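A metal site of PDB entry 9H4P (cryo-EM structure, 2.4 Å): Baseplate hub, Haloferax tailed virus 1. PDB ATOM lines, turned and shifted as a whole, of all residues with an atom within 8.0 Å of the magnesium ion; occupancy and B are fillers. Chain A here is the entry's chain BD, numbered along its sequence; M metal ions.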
ATOM      1  N   VAL A 387     -16.479 -24.383  23.830  1.00  0.00           N
ATOM      2  CA  VAL A 387     -16.070 -24.754  22.476  1.00  0.00           C
ATOM      3  C   VAL A 387     -16.456 -23.644  21.503  1.00  0.00           C
ATOM      4  O   VAL A 387     -17.618 -23.357  21.279  1.00  0.00           O
ATOM      5  CB  VAL A 387     -16.534 -26.157  22.075  1.00  0.00           C
ATOM      6  CG1 VAL A 387     -17.996 -26.444  22.382  1.00  0.00           C
ATOM      7  CG2 VAL A 387     -16.298 -26.430  20.595  1.00  0.00           C
ATOM      8  N   SER A 388     -15.442 -22.996  20.940  1.00  0.00           N
ATOM      9  CA  SER A 388     -15.558 -21.906  19.981  1.00  0.00           C
ATOM     10  C   SER A 388     -15.607 -22.479  18.571  1.00  0.00           C
ATOM     11  O   SER A 388     -14.621 -23.023  18.082  1.00  0.00           O
ATOM     12  CB  SER A 388     -14.342 -20.974  20.111  1.00  0.00           C
ATOM     13  OG  SER A 388     -14.251 -20.403  21.396  1.00  0.00           O
ATOM     14  N   VAL A 389     -16.760 -22.360  17.923  1.00  0.00           N
ATOM     15  CA  VAL A 389     -16.896 -22.589  16.477  1.00  0.00           C
ATOM     16  C   VAL A 389     -16.369 -21.371  15.743  1.00  0.00           C
ATOM     17  O   VAL A 389     -16.675 -20.253  16.127  1.00  0.00           O
ATOM     18  CB  VAL A 389     -18.378 -22.807  16.103  1.00  0.00           C
ATOM     19  CG1 VAL A 389     -18.524 -23.210  14.625  1.00  0.00           C
ATOM     20  CG2 VAL A 389     -19.051 -23.883  16.949  1.00  0.00           C
ATOM     21  N   ASP A 390     -15.650 -21.556  14.642  1.00  0.00           N
ATOM     22  CA  ASP A 390     -15.593 -20.582  13.551  1.00  0.00           C
ATOM     23  C   ASP A 390     -15.622 -21.275  12.188  1.00  0.00           C
ATOM     24  O   ASP A 390     -14.975 -22.299  11.982  1.00  0.00           O
ATOM     25  CB  ASP A 390     -14.376 -19.637  13.685  1.00  0.00           C
ATOM     26  CG  ASP A 390     -14.562 -18.517  14.735  1.00  0.00           C
ATOM     27  OD1 ASP A 390     -15.695 -18.009  14.918  1.00  0.00           O
ATOM     28  OD2 ASP A 390     -13.558 -18.148  15.379  1.00  0.00           O
ATOM     29  N   VAL A 391     -16.407 -20.730  11.256  1.00  0.00           N
ATOM     30  CA  VAL A 391     -16.595 -21.265   9.906  1.00  0.00           C
ATOM     31  C   VAL A 391     -16.021 -20.308   8.870  1.00  0.00           C
ATOM     32  O   VAL A 391     -16.335 -19.124   8.873  1.00  0.00           O
ATOM     33  CB  VAL A 391     -18.080 -21.545   9.611  1.00  0.00           C
ATOM     34  CG1 VAL A 391     -18.272 -22.130   8.208  1.00  0.00           C
ATOM     35  CG2 VAL A 391     -18.669 -22.525  10.629  1.00  0.00           C
ATOM     36  N   ALA A 398     -18.060 -16.789   8.344  1.00  0.00           N
ATOM     37  CA  ALA A 398     -19.473 -16.660   8.707  1.00  0.00           C
ATOM     38  C   ALA A 398     -19.714 -15.474   9.654  1.00  0.00           C
ATOM     39  O   ALA A 398     -18.876 -15.154  10.505  1.00  0.00           O
ATOM     40  CB  ALA A 398     -19.964 -17.970   9.296  1.00  0.00           C
ATOM     41  N   ASP A 399     -20.859 -14.823   9.521  1.00  0.00           N
ATOM     42  CA  ASP A 399     -21.227 -13.622  10.283  1.00  0.00           C
ATOM     43  C   ASP A 399     -21.892 -13.925  11.631  1.00  0.00           C
ATOM     44  O   ASP A 399     -21.845 -13.105  12.550  1.00  0.00           O
ATOM     45  CB  ASP A 399     -22.127 -12.757   9.406  1.00  0.00           C
ATOM     46  CG  ASP A 399     -21.377 -12.202   8.181  1.00  0.00           C
ATOM     47  OD1 ASP A 399     -20.364 -11.505   8.382  1.00  0.00           O
ATOM     48  OD2 ASP A 399     -21.840 -12.446   7.045  1.00  0.00           O
ATOM     49  N   ALA A 400     -22.477 -15.108  11.780  1.00  0.00           N
ATOM     50  CA  ALA A 400     -23.026 -15.628  13.030  1.00  0.00           C
ATOM     51  C   ALA A 400     -22.903 -17.154  13.059  1.00  0.00           C
ATOM     52  O   ALA A 400     -22.957 -17.810  12.019  1.00  0.00           O
ATOM     53  CB  ALA A 400     -24.477 -15.184  13.176  1.00  0.00           C
ATOM     54  N   ASP A 401     -22.787 -17.743  14.250  1.00  0.00           N
ATOM     55  CA  ASP A 401     -22.650 -19.185  14.464  1.00  0.00           C
ATOM     56  C   ASP A 401     -23.366 -19.655  15.739  1.00  0.00           C
ATOM     57  O   ASP A 401     -23.767 -18.859  16.597  1.00  0.00           O
ATOM     58  CB  ASP A 401     -21.175 -19.610  14.417  1.00  0.00           C
ATOM     59  CG  ASP A 401     -20.251 -18.934  15.440  1.00  0.00           C
ATOM     60  OD1 ASP A 401     -20.724 -18.469  16.482  1.00  0.00           O
ATOM     61  OD2 ASP A 401     -19.022 -18.854  15.197  1.00  0.00           O
ATOM     62  N   ARG A 402     -23.596 -20.962  15.833  1.00  0.00           N
ATOM     63  CA  ARG A 402     -24.104 -21.676  17.001  1.00  0.00           C
ATOM     64  C   ARG A 402     -23.437 -23.035  17.108  1.00  0.00           C
ATOM     65  O   ARG A 402     -23.306 -23.742  16.107  1.00  0.00           O
ATOM     66  CB  ARG A 402     -25.627 -21.858  16.884  1.00  0.00           C
ATOM     67  CG  ARG A 402     -26.444 -20.566  17.012  1.00  0.00           C
ATOM     68  CD  ARG A 402     -26.277 -19.935  18.398  1.00  0.00           C
ATOM     69  NE  ARG A 402     -27.188 -18.798  18.574  1.00  0.00           N
ATOM     70  CZ  ARG A 402     -27.037 -17.563  18.156  1.00  0.00           C
ATOM     71  NH1 ARG A 402     -27.970 -16.719  18.424  1.00  0.00           N
ATOM     72  NH2 ARG A 402     -26.005 -17.167  17.468  1.00  0.00           N
ATOM     73  N   PHE A 403     -23.117 -23.465  18.326  1.00  0.00           N
ATOM     74  CA  PHE A 403     -22.901 -24.865  18.695  1.00  0.00           C
ATOM     75  C   PHE A 403     -24.197 -25.380  19.315  1.00  0.00           C
ATOM     76  O   PHE A 403     -24.539 -25.019  20.437  1.00  0.00           O
ATOM     77  CB  PHE A 403     -21.705 -24.939  19.644  1.00  0.00           C
ATOM     78  CG  PHE A 403     -21.403 -26.305  20.194  1.00  0.00           C
ATOM     79  CD1 PHE A 403     -21.088 -27.369  19.338  1.00  0.00           C
ATOM     80  CD2 PHE A 403     -21.378 -26.510  21.586  1.00  0.00           C
ATOM     81  CE1 PHE A 403     -20.781 -28.624  19.862  1.00  0.00           C
ATOM     82  CE2 PHE A 403     -21.080 -27.774  22.117  1.00  0.00           C
ATOM     83  CZ  PHE A 403     -20.790 -28.838  21.243  1.00  0.00           C
ATOM     84  N   ALA A 488     -23.938 -22.059  11.026  1.00  0.00           N
ATOM     85  CA  ALA A 488     -23.362 -20.743  10.831  1.00  0.00           C
ATOM     86  C   ALA A 488     -23.929 -20.120   9.560  1.00  0.00           C
ATOM     87  O   ALA A 488     -24.384 -20.847   8.691  1.00  0.00           O
ATOM     88  CB  ALA A 488     -21.841 -20.868  10.787  1.00  0.00           C
ATOM     89  N   THR A 504     -13.824 -24.936  12.152  1.00  0.00           N
ATOM     90  CA  THR A 504     -12.820 -25.070  13.205  1.00  0.00           C
ATOM     91  C   THR A 504     -13.527 -25.135  14.541  1.00  0.00           C
ATOM     92  O   THR A 504     -14.361 -24.278  14.835  1.00  0.00           O
ATOM     93  CB  THR A 504     -11.862 -23.879  13.190  1.00  0.00           C
ATOM     94  OG1 THR A 504     -11.317 -23.681  11.905  1.00  0.00           O
ATOM     95  CG2 THR A 504     -10.698 -24.078  14.145  1.00  0.00           C
ATOM     96  N   SER A 952     -20.853 -22.771  24.252  1.00  0.00           N
ATOM     97  CA  SER A 952     -20.178 -21.884  23.298  1.00  0.00           C
ATOM     98  C   SER A 952     -19.793 -20.553  23.930  1.00  0.00           C
ATOM     99  O   SER A 952     -20.256 -20.200  25.017  1.00  0.00           O
ATOM    100  CB  SER A 952     -21.059 -21.670  22.067  1.00  0.00           C
ATOM    101  OG  SER A 952     -22.350 -21.179  22.405  1.00  0.00           O
ATOM    102  N   ASP A 953     -18.948 -19.797  23.259  1.00  0.00           N
ATOM    103  CA  ASP A 953     -18.701 -18.385  23.570  1.00  0.00           C
ATOM    104  C   ASP A 953     -19.814 -17.486  23.007  1.00  0.00           C
ATOM    105  O   ASP A 953     -20.331 -16.629  23.722  1.00  0.00           O
ATOM    106  CB  ASP A 953     -17.323 -17.962  23.037  1.00  0.00           C
ATOM    107  CG  ASP A 953     -16.963 -18.418  21.613  1.00  0.00           C
ATOM    108  OD1 ASP A 953     -17.827 -18.934  20.873  1.00  0.00           O
ATOM    109  OD2 ASP A 953     -15.762 -18.300  21.252  1.00  0.00           O
ATOM    110  N   ASN A 954     -20.201 -17.710  21.760  1.00  0.00           N
ATOM    111  CA  ASN A 954     -21.293 -17.047  21.039  1.00  0.00           C
ATOM    112  C   ASN A 954     -22.620 -17.785  21.205  1.00  0.00           C
ATOM    113  O   ASN A 954     -22.671 -19.014  20.968  1.00  0.00           O
ATOM    114  CB  ASN A 954     -20.864 -16.909  19.571  1.00  0.00           C
ATOM    115  CG  ASN A 954     -21.651 -15.878  18.775  1.00  0.00           C
ATOM    116  OD1 ASN A 954     -22.014 -14.816  19.261  1.00  0.00           O
ATOM    117  ND2 ASN A 954     -21.876 -16.126  17.512  1.00  0.00           N
ATOM    118  OXT ASN A 954     -23.604 -17.135  21.612  1.00  0.00           O
HETATM  119 MG    MG M   1     -17.374 -18.221  16.620  1.00  0.00          MG
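OD1 of Asp 401 is in hydrogen-bond range of ND2 of Asn 954, 2.8 Å away. The backbone NH (N) of Thr 504 is in hydrogen-bond range of the backbone carbonyl oxygen (O) of Asp 390 (2.9 Å).
Within 4 Å of the magnesium ion: Val 389, Asp 390 and Asp 401. The nearest printed residue that does not touch the magnesium ion is Asp 953 (4.3 Å).
The magnesium ion is bound by O of Val 389, OD2 of Asp 401 and OD1 of Asp 390.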
